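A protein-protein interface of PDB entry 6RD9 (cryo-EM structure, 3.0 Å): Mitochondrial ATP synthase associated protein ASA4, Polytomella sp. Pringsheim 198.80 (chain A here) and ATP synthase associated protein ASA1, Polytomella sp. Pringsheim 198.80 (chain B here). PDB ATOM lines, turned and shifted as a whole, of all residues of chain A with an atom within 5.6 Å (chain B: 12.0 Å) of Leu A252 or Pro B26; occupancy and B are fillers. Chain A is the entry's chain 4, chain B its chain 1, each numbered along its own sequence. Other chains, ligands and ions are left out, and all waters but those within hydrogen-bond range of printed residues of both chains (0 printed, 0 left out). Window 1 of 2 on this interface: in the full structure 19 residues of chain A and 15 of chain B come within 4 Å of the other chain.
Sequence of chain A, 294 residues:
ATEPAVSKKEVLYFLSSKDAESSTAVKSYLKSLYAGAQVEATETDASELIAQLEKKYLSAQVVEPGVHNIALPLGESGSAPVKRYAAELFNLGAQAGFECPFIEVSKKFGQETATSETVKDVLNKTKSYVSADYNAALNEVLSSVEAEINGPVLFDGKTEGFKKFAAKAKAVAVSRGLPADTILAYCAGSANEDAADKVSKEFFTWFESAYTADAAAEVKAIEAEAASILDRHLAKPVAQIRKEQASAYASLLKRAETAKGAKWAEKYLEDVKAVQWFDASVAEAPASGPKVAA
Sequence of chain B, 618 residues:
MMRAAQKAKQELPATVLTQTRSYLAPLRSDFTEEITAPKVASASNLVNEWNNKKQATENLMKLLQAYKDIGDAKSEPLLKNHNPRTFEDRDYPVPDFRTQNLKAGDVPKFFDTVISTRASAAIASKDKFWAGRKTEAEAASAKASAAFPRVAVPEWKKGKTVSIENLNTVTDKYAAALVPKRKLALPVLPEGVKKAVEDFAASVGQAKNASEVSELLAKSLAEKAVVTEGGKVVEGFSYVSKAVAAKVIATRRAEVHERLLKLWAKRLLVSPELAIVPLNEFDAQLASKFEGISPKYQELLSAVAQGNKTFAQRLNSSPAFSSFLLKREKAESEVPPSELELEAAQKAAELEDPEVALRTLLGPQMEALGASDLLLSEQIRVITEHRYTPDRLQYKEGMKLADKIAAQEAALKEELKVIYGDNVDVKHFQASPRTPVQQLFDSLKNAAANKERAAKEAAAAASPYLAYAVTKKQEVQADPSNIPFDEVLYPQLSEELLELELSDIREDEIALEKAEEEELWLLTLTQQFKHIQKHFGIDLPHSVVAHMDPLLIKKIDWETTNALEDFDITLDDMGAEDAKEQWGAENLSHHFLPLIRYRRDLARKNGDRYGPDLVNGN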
ATOM      1  N   SER A 247      -4.635 -18.422  21.086  1.00  0.00           N
ATOM      2  CA  SER A 247      -5.463 -19.263  20.234  1.00  0.00           C
ATOM      3  C   SER A 247      -5.326 -20.724  20.610  1.00  0.00           C
ATOM      4  O   SER A 247      -6.309 -21.468  20.592  1.00  0.00           O
ATOM      5  CB  SER A 247      -5.082 -19.076  18.774  1.00  0.00           C
ATOM      6  OG  SER A 247      -5.749 -20.023  17.967  1.00  0.00           O
ATOM      7  N   ALA A 248      -4.114 -21.156  20.942  1.00  0.00           N
ATOM      8  CA  ALA A 248      -3.904 -22.546  21.309  1.00  0.00           C
ATOM      9  C   ALA A 248      -4.400 -22.839  22.711  1.00  0.00           C
ATOM     10  O   ALA A 248      -4.807 -23.964  22.990  1.00  0.00           O
ATOM     11  CB  ALA A 248      -2.428 -22.906  21.189  1.00  0.00           C
ATOM     12  N   TYR A 249      -4.374 -21.856  23.600  1.00  0.00           N
ATOM     13  CA  TYR A 249      -4.893 -22.082  24.938  1.00  0.00           C
ATOM     14  C   TYR A 249      -6.403 -22.138  24.939  1.00  0.00           C
ATOM     15  O   TYR A 249      -6.989 -22.936  25.670  1.00  0.00           O
ATOM     16  CB  TYR A 249      -4.418 -20.981  25.874  1.00  0.00           C
ATOM     17  CG  TYR A 249      -5.018 -21.013  27.252  1.00  0.00           C
ATOM     18  CD1 TYR A 249      -4.542 -21.880  28.209  1.00  0.00           C
ATOM     19  CD2 TYR A 249      -6.037 -20.154  27.602  1.00  0.00           C
ATOM     20  CE1 TYR A 249      -5.076 -21.901  29.464  1.00  0.00           C
ATOM     21  CE2 TYR A 249      -6.576 -20.176  28.849  1.00  0.00           C
ATOM     22  CZ  TYR A 249      -6.093 -21.051  29.777  1.00  0.00           C
ATOM     23  OH  TYR A 249      -6.634 -21.069  31.035  1.00  0.00           O
ATOM     24  N   ALA A 250      -7.051 -21.291  24.146  1.00  0.00           N
ATOM     25  CA  ALA A 250      -8.502 -21.223  24.172  1.00  0.00           C
ATOM     26  C   ALA A 250      -9.132 -22.367  23.406  1.00  0.00           C
ATOM     27  O   ALA A 250     -10.229 -22.807  23.757  1.00  0.00           O
ATOM     28  CB  ALA A 250      -8.970 -19.892  23.605  1.00  0.00           C
ATOM     29  N   SER A 251      -8.458 -22.853  22.367  1.00  0.00           N
ATOM     30  CA  SER A 251      -8.944 -24.018  21.639  1.00  0.00           C
ATOM     31  C   SER A 251      -8.867 -25.269  22.492  1.00  0.00           C
ATOM     32  O   SER A 251      -9.695 -26.173  22.356  1.00  0.00           O
ATOM     33  CB  SER A 251      -8.133 -24.209  20.364  1.00  0.00           C
ATOM     34  OG  SER A 251      -8.503 -25.400  19.704  1.00  0.00           O
ATOM     35  N   LEU A 252      -7.880 -25.341  23.371  1.00  0.00           N
ATOM     36  CA  LEU A 252      -7.715 -26.495  24.232  1.00  0.00           C
ATOM     37  C   LEU A 252      -8.616 -26.444  25.453  1.00  0.00           C
ATOM     38  O   LEU A 252      -8.856 -27.486  26.062  1.00  0.00           O
ATOM     39  CB  LEU A 252      -6.264 -26.604  24.671  1.00  0.00           C
ATOM     40  CG  LEU A 252      -5.218 -27.454  23.968  1.00  0.00           C
ATOM     41  CD1 LEU A 252      -5.521 -28.891  24.236  1.00  0.00           C
ATOM     42  CD2 LEU A 252      -5.173 -27.196  22.492  1.00  0.00           C
ATOM     43  N   LEU A 253      -9.099 -25.264  25.841  1.00  0.00           N
ATOM     44  CA  LEU A 253     -10.108 -25.204  26.894  1.00  0.00           C
ATOM     45  C   LEU A 253     -11.450 -25.700  26.402  1.00  0.00           C
ATOM     46  O   LEU A 253     -12.136 -26.445  27.110  1.00  0.00           O
ATOM     47  CB  LEU A 253     -10.278 -23.788  27.421  1.00  0.00           C
ATOM     48  CG  LEU A 253      -9.421 -23.353  28.584  1.00  0.00           C
ATOM     49  CD1 LEU A 253      -9.761 -21.942  28.944  1.00  0.00           C
ATOM     50  CD2 LEU A 253      -9.747 -24.246  29.721  1.00  0.00           C
ATOM     51  N   LYS A 254     -11.852 -25.293  25.201  1.00  0.00           N
ATOM     52  CA  LYS A 254     -13.170 -25.680  24.726  1.00  0.00           C
ATOM     53  C   LYS A 254     -13.200 -27.134  24.295  1.00  0.00           C
ATOM     54  O   LYS A 254     -14.280 -27.711  24.163  1.00  0.00           O
ATOM     55  CB  LYS A 254     -13.630 -24.764  23.599  1.00  0.00           C
ATOM     56  CG  LYS A 254     -12.824 -24.833  22.335  1.00  0.00           C
ATOM     57  CD  LYS A 254     -13.419 -23.873  21.322  1.00  0.00           C
ATOM     58  CE  LYS A 254     -13.195 -22.430  21.764  1.00  0.00           C
ATOM     59  NZ  LYS A 254     -13.649 -21.430  20.759  1.00  0.00           N
ATOM     60  N   ARG A 255     -12.042 -27.751  24.075  1.00  0.00           N
ATOM     61  CA  ARG A 255     -12.035 -29.198  23.924  1.00  0.00           C
ATOM     62  C   ARG A 255     -12.294 -29.889  25.252  1.00  0.00           C
ATOM     63  O   ARG A 255     -12.754 -31.033  25.275  1.00  0.00           O
ATOM     64  CB  ARG A 255     -10.715 -29.670  23.329  1.00  0.00           C
ATOM     65  CG  ARG A 255     -10.823 -30.999  22.623  1.00  0.00           C
ATOM     66  CD  ARG A 255      -9.484 -31.476  22.136  1.00  0.00           C
ATOM     67  NE  ARG A 255      -8.783 -30.458  21.369  1.00  0.00           N
ATOM     68  CZ  ARG A 255      -7.535 -30.592  20.936  1.00  0.00           C
ATOM     69  NH1 ARG A 255      -6.957 -29.619  20.245  1.00  0.00           N
ATOM     70  NH2 ARG A 255      -6.860 -31.702  21.199  1.00  0.00           N
ATOM     71  N   ALA A 256     -12.005 -29.222  26.361  1.00  0.00           N
ATOM     72  CA  ALA A 256     -12.361 -29.748  27.668  1.00  0.00           C
ATOM     73  C   ALA A 256     -13.711 -29.257  28.151  1.00  0.00           C
ATOM     74  O   ALA A 256     -14.259 -29.831  29.093  1.00  0.00           O
ATOM     75  CB  ALA A 256     -11.298 -29.380  28.699  1.00  0.00           C
ATOM     76  N   TYR A 268      -9.422 -31.925  33.948  1.00  0.00           N
ATOM     77  CA  TYR A 268      -8.696 -30.911  33.190  1.00  0.00           C
ATOM     78  C   TYR A 268      -9.005 -29.520  33.709  1.00  0.00           C
ATOM     79  O   TYR A 268      -8.097 -28.745  34.014  1.00  0.00           O
ATOM     80  CB  TYR A 268      -9.070 -31.006  31.721  1.00  0.00           C
ATOM     81  CG  TYR A 268      -8.019 -30.561  30.752  1.00  0.00           C
ATOM     82  CD1 TYR A 268      -8.010 -29.274  30.257  1.00  0.00           C
ATOM     83  CD2 TYR A 268      -7.062 -31.441  30.300  1.00  0.00           C
ATOM     84  CE1 TYR A 268      -7.063 -28.873  29.358  1.00  0.00           C
ATOM     85  CE2 TYR A 268      -6.113 -31.047  29.405  1.00  0.00           C
ATOM     86  CZ  TYR A 268      -6.118 -29.767  28.938  1.00  0.00           C
ATOM     87  OH  TYR A 268      -5.160 -29.395  28.043  1.00  0.00           O
ATOM     88  N   TYR B  23      -0.490 -22.920  28.538  1.00  0.00           N
ATOM     89  CA  TYR B  23       0.429 -23.729  29.313  1.00  0.00           C
ATOM     90  C   TYR B  23      -0.007 -25.167  29.299  1.00  0.00           C
ATOM     91  O   TYR B  23       0.731 -26.049  29.700  1.00  0.00           O
ATOM     92  CB  TYR B  23       0.522 -23.229  30.748  1.00  0.00           C
ATOM     93  CG  TYR B  23      -0.798 -23.015  31.438  1.00  0.00           C
ATOM     94  CD1 TYR B  23      -1.371 -21.763  31.479  1.00  0.00           C
ATOM     95  CD2 TYR B  23      -1.456 -24.055  32.068  1.00  0.00           C
ATOM     96  CE1 TYR B  23      -2.557 -21.557  32.107  1.00  0.00           C
ATOM     97  CE2 TYR B  23      -2.643 -23.856  32.693  1.00  0.00           C
ATOM     98  CZ  TYR B  23      -3.188 -22.604  32.708  1.00  0.00           C
ATOM     99  OH  TYR B  23      -4.380 -22.387  33.339  1.00  0.00           O
ATOM    100  N   LEU B  24      -1.230 -25.399  28.869  1.00  0.00           N
ATOM    101  CA  LEU B  24      -1.812 -26.726  28.907  1.00  0.00           C
ATOM    102  C   LEU B  24      -1.656 -27.453  27.581  1.00  0.00           C
ATOM    103  O   LEU B  24      -1.573 -26.843  26.516  1.00  0.00           O
ATOM    104  CB  LEU B  24      -3.275 -26.647  29.340  1.00  0.00           C
ATOM    105  CG  LEU B  24      -4.104 -25.437  28.951  1.00  0.00           C
ATOM    106  CD1 LEU B  24      -4.484 -25.477  27.550  1.00  0.00           C
ATOM    107  CD2 LEU B  24      -5.338 -25.466  29.786  1.00  0.00           C
ATOM    108  N   ALA B  25      -1.611 -28.767  27.668  1.00  0.00           N
ATOM    109  CA  ALA B  25      -1.224 -29.646  26.588  1.00  0.00           C
ATOM    110  C   ALA B  25      -2.409 -30.463  26.100  1.00  0.00           C
ATOM    111  O   ALA B  25      -3.394 -30.637  26.823  1.00  0.00           O
ATOM    112  CB  ALA B  25      -0.109 -30.583  27.068  1.00  0.00           C
ATOM    113  N   PRO B  26      -2.365 -30.962  24.867  1.00  0.00           N
ATOM    114  CA  PRO B  26      -3.359 -31.952  24.451  1.00  0.00           C
ATOM    115  C   PRO B  26      -3.125 -33.277  25.154  1.00  0.00           C
ATOM    116  O   PRO B  26      -1.998 -33.768  25.226  1.00  0.00           O
ATOM    117  CB  PRO B  26      -3.134 -32.071  22.943  1.00  0.00           C
ATOM    118  CG  PRO B  26      -1.774 -31.580  22.730  1.00  0.00           C
ATOM    119  CD  PRO B  26      -1.554 -30.510  23.731  1.00  0.00           C
ATOM    120  N   LEU B  27      -4.195 -33.848  25.685  1.00  0.00           N
ATOM    121  CA  LEU B  27      -4.100 -35.134  26.352  1.00  0.00           C
ATOM    122  C   LEU B  27      -4.084 -36.251  25.321  1.00  0.00           C
ATOM    123  O   LEU B  27      -4.899 -36.264  24.397  1.00  0.00           O
ATOM    124  CB  LEU B  27      -5.264 -35.317  27.316  1.00  0.00           C
ATOM    125  CG  LEU B  27      -5.297 -34.479  28.583  1.00  0.00           C
ATOM    126  CD1 LEU B  27      -6.333 -35.022  29.521  1.00  0.00           C
ATOM    127  CD2 LEU B  27      -3.953 -34.461  29.245  1.00  0.00           C
ATOM    128  N   ARG B  28      -3.157 -37.185  25.476  1.00  0.00           N
ATOM    129  CA  ARG B  28      -3.007 -38.298  24.555  1.00  0.00           C
ATOM    130  C   ARG B  28      -3.037 -39.599  25.333  1.00  0.00           C
ATOM    131  O   ARG B  28      -2.511 -39.680  26.443  1.00  0.00           O
ATOM    132  CB  ARG B  28      -1.711 -38.193  23.769  1.00  0.00           C
ATOM    133  CG  ARG B  28      -1.700 -37.047  22.798  1.00  0.00           C
ATOM    134  CD  ARG B  28      -0.324 -36.780  22.261  1.00  0.00           C
ATOM    135  NE  ARG B  28       0.322 -38.000  21.810  1.00  0.00           N
ATOM    136  CZ  ARG B  28       1.461 -38.019  21.140  1.00  0.00           C
ATOM    137  NH1 ARG B  28       1.991 -39.168  20.767  1.00  0.00           N
ATOM    138  NH2 ARG B  28       2.062 -36.886  20.841  1.00  0.00           N
ATOM    139  N   SER B  29      -3.667 -40.611  24.751  1.00  0.00           N
ATOM    140  CA  SER B  29      -3.757 -41.936  25.351  1.00  0.00           C
ATOM    141  C   SER B  29      -3.376 -42.937  24.275  1.00  0.00           C
ATOM    142  O   SER B  29      -4.246 -43.552  23.658  1.00  0.00           O
ATOM    143  CB  SER B  29      -5.144 -42.194  25.876  1.00  0.00           C
ATOM    144  OG  SER B  29      -6.071 -42.268  24.813  1.00  0.00           O
ATOM    145  N   ASP B  30      -2.081 -43.107  24.059  1.00  0.00           N
ATOM    146  CA  ASP B  30      -1.590 -44.052  23.078  1.00  0.00           C
ATOM    147  C   ASP B  30      -0.221 -44.522  23.518  1.00  0.00           C
ATOM    148  O   ASP B  30       0.470 -43.844  24.278  1.00  0.00           O
ATOM    149  CB  ASP B  30      -1.510 -43.453  21.678  1.00  0.00           C
ATOM    150  CG  ASP B  30      -0.476 -42.369  21.571  1.00  0.00           C
ATOM    151  OD1 ASP B  30      -0.622 -41.356  22.270  1.00  0.00           O
ATOM    152  OD2 ASP B  30       0.494 -42.527  20.808  1.00  0.00           O
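The side-chain hydroxyl (OH) of Tyr B23 is in hydrogen-bond range of the side-chain hydroxyl (OH) of Tyr A249 (3.5 Å).
The side-chain hydroxyl of Tyr A268 is in hydrogen-bond range of the backbone carbonyl oxygen of Ala B25, 2.5 Å away.
Among the printed residues, merely in contact across the chains: Leu A252 with Leu B24 (3.6 Å), Tyr A268 with Leu B24 (3.6 Å), Tyr A249 with Leu B24 (3.6 Å), Tyr A268 with Leu B27 (3.6 Å), Leu A252 with Pro B26 (3.8 Å) and Leu A252 with Ala B25 (3.8 Å).
Of the printed residues of chain B, Leu A252 touches Leu B24 (3.6 Å), Ala B25 (3.8 Å) and Pro B26 (3.8 Å).
Pro B26 touches just one residue of chain A: Leu A252 (3.8 Å).
No residue of chain B comes within 4 Å of Ser A251.
No residue of chain B comes within 4 Å of Lys A254.
No residue of chain B comes within 4 Å of Arg A255.
No residue of chain B comes within 4 Å of Ala A256.
Printed residues of chain A within 4 Å of Leu B27: Tyr A268.
Of the printed residues of chain B, Tyr A268 touches Leu B24, Ala B25 and Leu B27.
Arg B28 touches none of the printed residues of chain A.
The nearest residue of chain B that does not touch Leu A252 is Leu B27 (5.3 Å).
Of the 8 printed residues of chain B, 5 touch a printed residue of chain A.
Hydrophobic or aromatic side chains of chain B that line the printed part of chain A: Tyr B23, Leu B24 and Leu B27.
Among the printed residues, 8 pairs touch across the chains.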
